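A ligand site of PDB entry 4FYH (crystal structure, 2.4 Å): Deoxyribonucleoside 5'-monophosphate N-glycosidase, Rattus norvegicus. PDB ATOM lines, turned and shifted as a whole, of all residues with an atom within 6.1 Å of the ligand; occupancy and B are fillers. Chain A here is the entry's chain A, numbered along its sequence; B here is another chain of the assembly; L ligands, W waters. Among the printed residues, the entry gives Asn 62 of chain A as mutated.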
ATOM      1  N   TYR A   6     -34.071  25.407  21.144  1.00  0.00           N
ATOM      2  CA  TYR A   6     -32.849  24.633  21.201  1.00  0.00           C
ATOM      3  C   TYR A   6     -31.763  25.547  21.762  1.00  0.00           C
ATOM      4  O   TYR A   6     -31.491  26.599  21.184  1.00  0.00           O
ATOM      5  CB  TYR A   6     -32.467  24.159  19.795  1.00  0.00           C
ATOM      6  CG  TYR A   6     -31.326  23.161  19.744  1.00  0.00           C
ATOM      7  CD1 TYR A   6     -31.564  21.846  19.373  1.00  0.00           C
ATOM      8  CD2 TYR A   6     -30.023  23.543  20.048  1.00  0.00           C
ATOM      9  CE1 TYR A   6     -30.526  20.920  19.304  1.00  0.00           C
ATOM     10  CE2 TYR A   6     -28.977  22.624  19.986  1.00  0.00           C
ATOM     11  CZ  TYR A   6     -29.239  21.305  19.620  1.00  0.00           C
ATOM     12  OH  TYR A   6     -28.212  20.392  19.549  1.00  0.00           O
ATOM     13  N   PHE A   7     -31.153  25.155  22.880  1.00  0.00           N
ATOM     14  CA  PHE A   7     -30.074  25.956  23.470  1.00  0.00           C
ATOM     15  C   PHE A   7     -28.703  25.313  23.266  1.00  0.00           C
ATOM     16  O   PHE A   7     -28.529  24.113  23.519  1.00  0.00           O
ATOM     17  CB  PHE A   7     -30.313  26.241  24.964  1.00  0.00           C
ATOM     18  CG  PHE A   7     -29.142  26.930  25.636  1.00  0.00           C
ATOM     19  CD1 PHE A   7     -28.219  26.190  26.378  1.00  0.00           C
ATOM     20  CD2 PHE A   7     -28.943  28.292  25.497  1.00  0.00           C
ATOM     21  CE1 PHE A   7     -27.126  26.809  26.977  1.00  0.00           C
ATOM     22  CE2 PHE A   7     -27.851  28.932  26.089  1.00  0.00           C
ATOM     23  CZ  PHE A   7     -26.944  28.186  26.829  1.00  0.00           C
ATOM     24  N   CYS A   8     -27.758  26.129  22.808  1.00  0.00           N
ATOM     25  CA  CYS A   8     -26.361  25.698  22.585  1.00  0.00           C
ATOM     26  C   CYS A   8     -25.408  26.388  23.553  1.00  0.00           C
ATOM     27  O   CYS A   8     -25.467  27.596  23.726  1.00  0.00           O
ATOM     28  CB  CYS A   8     -25.885  26.009  21.158  1.00  0.00           C
ATOM     29  SG  CYS A   8     -27.103  25.799  19.845  1.00  0.00           S
ATOM     30  N   GLY A   9     -24.518  25.600  24.141  1.00  0.00           N
ATOM     31  CA  GLY A   9     -23.442  26.134  24.988  1.00  0.00           C
ATOM     32  C   GLY A   9     -22.285  25.150  25.032  1.00  0.00           C
ATOM     33  O   GLY A   9     -22.496  23.935  24.870  1.00  0.00           O
ATOM     34  N   SER A  10     -21.070  25.663  25.204  1.00  0.00           N
ATOM     35  CA  SER A  10     -19.862  24.841  25.260  1.00  0.00           C
ATOM     36  C   SER A  10     -19.970  23.760  26.334  1.00  0.00           C
ATOM     37  O   SER A  10     -20.451  24.021  27.431  1.00  0.00           O
ATOM     38  CB  SER A  10     -18.647  25.748  25.516  1.00  0.00           C
ATOM     39  OG  SER A  10     -17.429  25.006  25.559  1.00  0.00           O
ATOM     40  N   ILE A  11     -19.540  22.545  26.004  1.00  0.00           N
ATOM     41  CA  ILE A  11     -19.323  21.479  26.987  1.00  0.00           C
ATOM     42  C   ILE A  11     -17.861  21.034  26.942  1.00  0.00           C
ATOM     43  O   ILE A  11     -17.090  21.331  27.861  1.00  0.00           O
ATOM     44  CB  ILE A  11     -20.275  20.267  26.776  1.00  0.00           C
ATOM     45  CG1 ILE A  11     -21.741  20.712  26.863  1.00  0.00           C
ATOM     46  CG2 ILE A  11     -19.981  19.178  27.810  1.00  0.00           C
ATOM     47  CD1 ILE A  11     -22.739  19.700  26.326  1.00  0.00           C
ATOM     48  N   ARG A  12     -17.478  20.364  25.871  1.00  0.00           N
ATOM     49  CA  ARG A  12     -16.124  19.860  25.714  1.00  0.00           C
ATOM     50  C   ARG A  12     -15.124  20.949  25.333  1.00  0.00           C
ATOM     51  O   ARG A  12     -13.913  20.710  25.337  1.00  0.00           O
ATOM     52  CB  ARG A  12     -16.104  18.718  24.690  1.00  0.00           C
ATOM     53  CG  ARG A  12     -15.231  17.565  25.100  1.00  0.00           C
ATOM     54  CD  ARG A  12     -15.905  16.697  26.158  1.00  0.00           C
ATOM     55  NE  ARG A  12     -14.964  16.297  27.200  1.00  0.00           N
ATOM     56  CZ  ARG A  12     -15.045  15.156  27.893  1.00  0.00           C
ATOM     57  NH1 ARG A  12     -16.005  14.282  27.630  1.00  0.00           N
ATOM     58  NH2 ARG A  12     -14.144  14.875  28.815  1.00  0.00           N
ATOM     59  N   GLY A  13     -15.618  22.138  25.001  1.00  0.00           N
ATOM     60  CA  GLY A  13     -14.749  23.292  24.761  1.00  0.00           C
ATOM     61  C   GLY A  13     -14.408  24.022  26.050  1.00  0.00           C
ATOM     62  O   GLY A  13     -13.623  24.974  26.043  1.00  0.00           O
ATOM     63  N   GLY A  14     -14.989  23.573  27.153  1.00  0.00           N
ATOM     64  CA  GLY A  14     -14.824  24.207  28.450  1.00  0.00           C
ATOM     65  C   GLY A  14     -16.152  24.534  29.094  1.00  0.00           C
ATOM     66  O   GLY A  14     -17.062  25.049  28.454  1.00  0.00           O
ATOM     67  N   THR A  36     -32.971  20.870  24.974  1.00  0.00           N
ATOM     68  CA  THR A  36     -31.643  20.511  25.462  1.00  0.00           C
ATOM     69  C   THR A  36     -31.514  20.744  26.970  1.00  0.00           C
ATOM     70  O   THR A  36     -31.491  21.888  27.438  1.00  0.00           O
ATOM     71  CB  THR A  36     -30.563  21.349  24.728  1.00  0.00           C
ATOM     72  OG1 THR A  36     -31.040  22.685  24.547  1.00  0.00           O
ATOM     73  CG2 THR A  36     -30.259  20.750  23.363  1.00  0.00           C
ATOM     74  N   ASP A  55     -20.996   8.896  21.011  1.00  0.00           N
ATOM     75  CA  ASP A  55     -21.089  10.208  20.390  1.00  0.00           C
ATOM     76  C   ASP A  55     -22.096  10.235  19.243  1.00  0.00           C
ATOM     77  O   ASP A  55     -22.786  11.237  19.053  1.00  0.00           O
ATOM     78  CB  ASP A  55     -19.701  10.660  19.942  1.00  0.00           C
ATOM     79  CG  ASP A  55     -18.712  10.731  21.101  1.00  0.00           C
ATOM     80  OD1 ASP A  55     -17.509  10.479  20.890  1.00  0.00           O
ATOM     81  OD2 ASP A  55     -19.136  11.027  22.239  1.00  0.00           O
ATOM     82  N   ILE A  58     -25.554  10.835  20.553  1.00  0.00           N
ATOM     83  CA  ILE A  58     -25.664  12.238  20.955  1.00  0.00           C
ATOM     84  C   ILE A  58     -25.925  13.167  19.754  1.00  0.00           C
ATOM     85  O   ILE A  58     -26.804  14.018  19.800  1.00  0.00           O
ATOM     86  CB  ILE A  58     -24.426  12.706  21.778  1.00  0.00           C
ATOM     87  CG1 ILE A  58     -24.537  12.198  23.212  1.00  0.00           C
ATOM     88  CG2 ILE A  58     -24.299  14.230  21.772  1.00  0.00           C
ATOM     89  CD1 ILE A  58     -23.198  11.883  23.843  1.00  0.00           C
ATOM     90  N   ASN A  62     -29.442  15.079  18.996  1.00  0.00           N
ATOM     91  CA  ASN A  62     -29.373  16.530  18.863  1.00  0.00           C
ATOM     92  C   ASN A  62     -29.861  17.070  17.509  1.00  0.00           C
ATOM     93  O   ASN A  62     -30.546  18.097  17.462  1.00  0.00           O
ATOM     94  CB  ASN A  62     -27.974  17.049  19.191  1.00  0.00           C
ATOM     95  CG  ASN A  62     -27.700  17.116  20.702  1.00  0.00           C
ATOM     96  OD1 ASN A  62     -28.592  16.919  21.527  1.00  0.00           O
ATOM     97  ND2 ASN A  62     -26.453  17.397  21.050  1.00  0.00           N
ATOM     98  N   PRO A  79     -15.310  29.297  23.185  1.00  0.00           N
ATOM     99  CA  PRO A  79     -15.111  28.643  21.887  1.00  0.00           C
ATOM    100  C   PRO A  79     -15.430  27.151  21.971  1.00  0.00           C
ATOM    101  O   PRO A  79     -15.049  26.496  22.942  1.00  0.00           O
ATOM    102  CB  PRO A  79     -13.627  28.897  21.586  1.00  0.00           C
ATOM    103  CG  PRO A  79     -13.227  30.027  22.467  1.00  0.00           C
ATOM    104  CD  PRO A  79     -14.063  29.886  23.710  1.00  0.00           C
ATOM    105  N   SER A  80     -16.133  26.641  20.960  1.00  0.00           N
ATOM    106  CA  SER A  80     -16.637  25.275  20.972  1.00  0.00           C
ATOM    107  C   SER A  80     -17.018  24.778  19.578  1.00  0.00           C
ATOM    108  O   SER A  80     -17.808  25.407  18.873  1.00  0.00           O
ATOM    109  CB  SER A  80     -17.832  25.161  21.932  1.00  0.00           C
ATOM    110  OG  SER A  80     -18.607  24.005  21.677  1.00  0.00           O
ATOM    111  N   LEU A  81     -16.456  23.642  19.192  1.00  0.00           N
ATOM    112  CA  LEU A  81     -16.758  22.983  17.929  1.00  0.00           C
ATOM    113  C   LEU A  81     -18.241  22.669  17.817  1.00  0.00           C
ATOM    114  O   LEU A  81     -18.852  22.965  16.793  1.00  0.00           O
ATOM    115  CB  LEU A  81     -15.971  21.671  17.853  1.00  0.00           C
ATOM    116  CG  LEU A  81     -14.625  21.455  17.132  1.00  0.00           C
ATOM    117  CD1 LEU A  81     -13.917  22.693  16.639  1.00  0.00           C
ATOM    118  CD2 LEU A  81     -13.718  20.612  18.015  1.00  0.00           C
ATOM    119  N   GLY A  82     -18.814  22.074  18.865  1.00  0.00           N
ATOM    120  CA  GLY A  82     -20.213  21.638  18.877  1.00  0.00           C
ATOM    121  C   GLY A  82     -21.209  22.758  18.681  1.00  0.00           C
ATOM    122  O   GLY A  82     -22.123  22.645  17.851  1.00  0.00           O
ATOM    123  N   VAL A  83     -21.024  23.859  19.423  1.00  0.00           N
ATOM    124  CA  VAL A  83     -21.872  25.059  19.300  1.00  0.00           C
ATOM    125  C   VAL A  83     -21.810  25.612  17.889  1.00  0.00           C
ATOM    126  O   VAL A  83     -22.845  25.881  17.271  1.00  0.00           O
ATOM    127  CB  VAL A  83     -21.452  26.180  20.304  1.00  0.00           C
ATOM    128  CG1 VAL A  83     -22.295  27.444  20.103  1.00  0.00           C
ATOM    129  CG2 VAL A  83     -21.601  25.694  21.734  1.00  0.00           C
ATOM    130  N   GLU A  86     -23.671  23.213  15.494  1.00  0.00           N
ATOM    131  CA  GLU A  86     -25.114  23.377  15.698  1.00  0.00           C
ATOM    132  C   GLU A  86     -25.640  24.647  15.014  1.00  0.00           C
ATOM    133  O   GLU A  86     -26.699  24.622  14.381  1.00  0.00           O
ATOM    134  CB  GLU A  86     -25.424  23.391  17.207  1.00  0.00           C
ATOM    135  CG  GLU A  86     -25.266  22.017  17.879  1.00  0.00           C
ATOM    136  CD  GLU A  86     -25.369  22.065  19.404  1.00  0.00           C
ATOM    137  OE1 GLU A  86     -25.885  21.072  19.990  1.00  0.00           O
ATOM    138  OE2 GLU A  86     -24.949  23.062  20.032  1.00  0.00           O
ATOM    139  N   LEU B 109     -12.619  14.720  21.951  1.00  0.00           N
ATOM    140  CA  LEU B 109     -13.226  15.454  20.825  1.00  0.00           C
ATOM    141  C   LEU B 109     -14.719  15.674  21.031  1.00  0.00           C
ATOM    142  O   LEU B 109     -15.434  14.782  21.487  1.00  0.00           O
ATOM    143  CB  LEU B 109     -12.958  14.761  19.478  1.00  0.00           C
ATOM    144  CG  LEU B 109     -13.628  15.382  18.232  1.00  0.00           C
ATOM    145  CD1 LEU B 109     -13.222  16.821  18.030  1.00  0.00           C
ATOM    146  CD2 LEU B 109     -13.299  14.564  16.999  1.00  0.00           C
ATOM    147  N   SER B 110     -15.163  16.880  20.691  1.00  0.00           N
ATOM    148  CA  SER B 110     -16.577  17.230  20.663  1.00  0.00           C
ATOM    149  C   SER B 110     -17.435  16.052  20.171  1.00  0.00           C
ATOM    150  O   SER B 110     -17.204  15.497  19.104  1.00  0.00           O
ATOM    151  CB  SER B 110     -16.793  18.429  19.751  1.00  0.00           C
ATOM    152  OG  SER B 110     -18.139  18.842  19.738  1.00  0.00           O
ATOM    153  N   ALA B 111     -18.425  15.686  20.978  1.00  0.00           N
ATOM    154  CA  ALA B 111     -19.377  14.645  20.617  1.00  0.00           C
ATOM    155  C   ALA B 111     -20.068  14.952  19.284  1.00  0.00           C
ATOM    156  O   ALA B 111     -20.348  14.045  18.495  1.00  0.00           O
ATOM    157  CB  ALA B 111     -20.408  14.459  21.717  1.00  0.00           C
ATOM    158  N   MET B 112     -20.330  16.239  19.043  1.00  0.00           N
ATOM    159  CA  MET B 112     -21.028  16.669  17.823  1.00  0.00           C
ATOM    160  C   MET B 112     -20.208  16.462  16.558  1.00  0.00           C
ATOM    161  O   MET B 112     -20.773  16.257  15.490  1.00  0.00           O
ATOM    162  CB  MET B 112     -21.490  18.117  17.927  1.00  0.00           C
ATOM    163  CG  MET B 112     -22.602  18.320  18.953  1.00  0.00           C
ATOM    164  SD  MET B 112     -24.017  17.242  18.667  1.00  0.00           S
ATOM    165  CE  MET B 112     -24.847  18.097  17.331  1.00  0.00           C
ATOM    166  N   ILE B 113     -18.887  16.531  16.694  1.00  0.00           N
ATOM    167  CA  ILE B 113     -17.990  16.266  15.573  1.00  0.00           C
ATOM    168  C   ILE B 113     -17.750  14.768  15.422  1.00  0.00           C
ATOM    169  O   ILE B 113     -17.928  14.204  14.343  1.00  0.00           O
ATOM    170  CB  ILE B 113     -16.641  17.045  15.696  1.00  0.00           C
ATOM    171  CG1 ILE B 113     -16.873  18.550  15.934  1.00  0.00           C
ATOM    172  CG2 ILE B 113     -15.757  16.798  14.474  1.00  0.00           C
ATOM    173  CD1 ILE B 113     -17.783  19.264  14.880  1.00  0.00           C
HETATM  174  O1  LIG L   1     -18.513  22.194  23.354  1.00  0.00           O
HETATM  175  P1  LIG L   1     -18.763  20.843  22.548  1.00  0.00           P
HETATM  176  O2  LIG L   1     -17.870  20.799  21.369  1.00  0.00           O
HETATM  177  O3  LIG L   1     -18.744  19.718  23.501  1.00  0.00           O
HETATM  178  O4  LIG L   1     -20.279  21.027  22.032  1.00  0.00           O
HETATM  179  C1  LIG L   1     -21.289  21.548  22.904  1.00  0.00           C
HETATM  180  C2  LIG L   1     -22.602  21.640  22.135  1.00  0.00           C
HETATM  181  O5  LIG L   1     -22.768  20.397  21.445  1.00  0.00           O
HETATM  182  C3  LIG L   1     -23.762  21.785  23.119  1.00  0.00           C
HETATM  183  O6  LIG L   1     -24.544  22.942  22.769  1.00  0.00           O
HETATM  184  C4  LIG L   1     -24.559  20.474  23.047  1.00  0.00           C
HETATM  185  O7  LIG L   1     -25.906  20.703  22.594  1.00  0.00           O
HETATM  186  C5  LIG L   1     -23.752  19.545  22.090  1.00  0.00           C
HETATM  187  N1  LIG L   1     -23.022  18.484  22.875  1.00  0.00           N
HETATM  188  C6  LIG L   1     -21.686  18.341  23.000  1.00  0.00           C
HETATM  189  C7  LIG L   1     -21.447  17.305  23.807  1.00  0.00           C
HETATM  190  C8  LIG L   1     -22.632  16.829  24.172  1.00  0.00           C
HETATM  191  C9  LIG L   1     -23.614  17.540  23.609  1.00  0.00           C
HETATM  192  N2  LIG L   1     -24.899  17.210  23.855  1.00  0.00           N
HETATM  193  C10 LIG L   1     -25.246  16.077  24.752  1.00  0.00           C
HETATM  194  N3  LIG L   1     -24.032  15.395  25.299  1.00  0.00           N
HETATM  195  C11 LIG L   1     -22.784  15.799  24.985  1.00  0.00           C
HETATM  196  N4  LIG L   1     -21.668  15.189  25.470  1.00  0.00           N
HETATM  197  C12 LIG L   1     -21.776  14.018  26.381  1.00  0.00           C
HETATM  198  N5  LIG L   1     -20.480  15.631  25.120  1.00  0.00           N
HETATM  199  C13 LIG L   1     -20.355  16.690  24.298  1.00  0.00           C
HETATM  200  N6  LIG L   1     -19.160  17.173  23.927  1.00  0.00           N
HETATM  201  O   HOH W   1     -15.330  21.800  21.214  1.00  0.00           O
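N6 of the ligand sits close to N of Ala 111 of chain B.
Tyr 6 touches the ligand.
CA of Cys 8 touches O6 of the ligand (3.3 Å).
Ser 10 touches the ligand (CA to O1, 3.5 Å).
Ile 58 touches the ligand (CD1 to C12, 3.6 Å).
N of Leu 81 touches O2 of the ligand, at 3.8 Å.
Val 83 touches the ligand.
Met 112 of chain B touches the ligand.
Hydrophobic or aromatic side chains that line the ligand: Ile 11, Ile 58, Ala 111 of chain B and Met 112 of chain B.
17 residues have an atom within 4 Å of the ligand: Tyr 6, Cys 8, Gly 9, Ser 10, Ile 11, Arg 12, Gly 13, Ile 58, Asn 62, Ser 80, Leu 81, Gly 82, Val 83, Glu 86, Ser 110 of chain B, Ala 111 of chain B and Met 112 of chain B.
Water W1 lies within hydrogen-bond range of an oxygen (O2) of the ligand (2.7 Å) and the backbone NH of Leu 81 (3.0 Å).
OG of Ser 80 sits close to N of Gly 82, 3.4 Å away.
The side-chain amide nitrogen (ND2) of Asn 62 sits at hydrogen-bond distance from the side-chain sulfur (SD) of Met 112 of chain B (3.4 Å).
OH of Tyr 6 lies within hydrogen-bond range of OE1 of Glu 86, 2.5 Å away.
N of Val 83 sits at hydrogen-bond distance from OG of Ser 80 (3.3 Å).
OG of Ser 10 sits close to N of Gly 13.
The backbone carbonyl oxygen (O) of Gly 14 is in hydrogen-bond range of the side-chain hydroxyl (OG) of Ser 10.
OG of Ser 110 of chain B lies within hydrogen-bond range of N of Gly 82 (3.4 Å).
The side-chain carboxylate (OE2) of Glu 86 lies close to the side-chain sulfur (SG) of Cys 8 (3.5 Å).
The backbone NH of Gly 13 sits at hydrogen-bond distance from an oxygen (O1) of the ligand (3.3 Å).
The backbone carbonyl oxygen (O) of Gly 9 sits close to an oxygen (O6) of the ligand, 3.1 Å away.
An oxygen (O3) of the ligand is in hydrogen-bond range of the backbone NH (N) of Arg 12 (2.8 Å).
The side-chain amide nitrogen (ND2) of Asn 62 is in hydrogen-bond range of a nitrogen (N2) of the ligand.
The backbone NH (N) of Gly 9 lies within hydrogen-bond range of an oxygen (O6) of the ligand.
The side-chain carboxylate (OE1) of Glu 86 lies within hydrogen-bond range of an oxygen (O7) of the ligand (2.6 Å).
N of Gly 82 sits at hydrogen-bond distance from O2 of the ligand (3.0 Å).
The backbone NH (N) of Ile 11 is in hydrogen-bond range of an oxygen (O1) of the ligand.
An oxygen (O1) of the ligand sits at hydrogen-bond distance from the side-chain hydroxyl (OG) of Ser 80 (2.5 Å).
OG of Ser 110 of chain B sits at hydrogen-bond distance from O2 of the ligand (2.6 Å).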
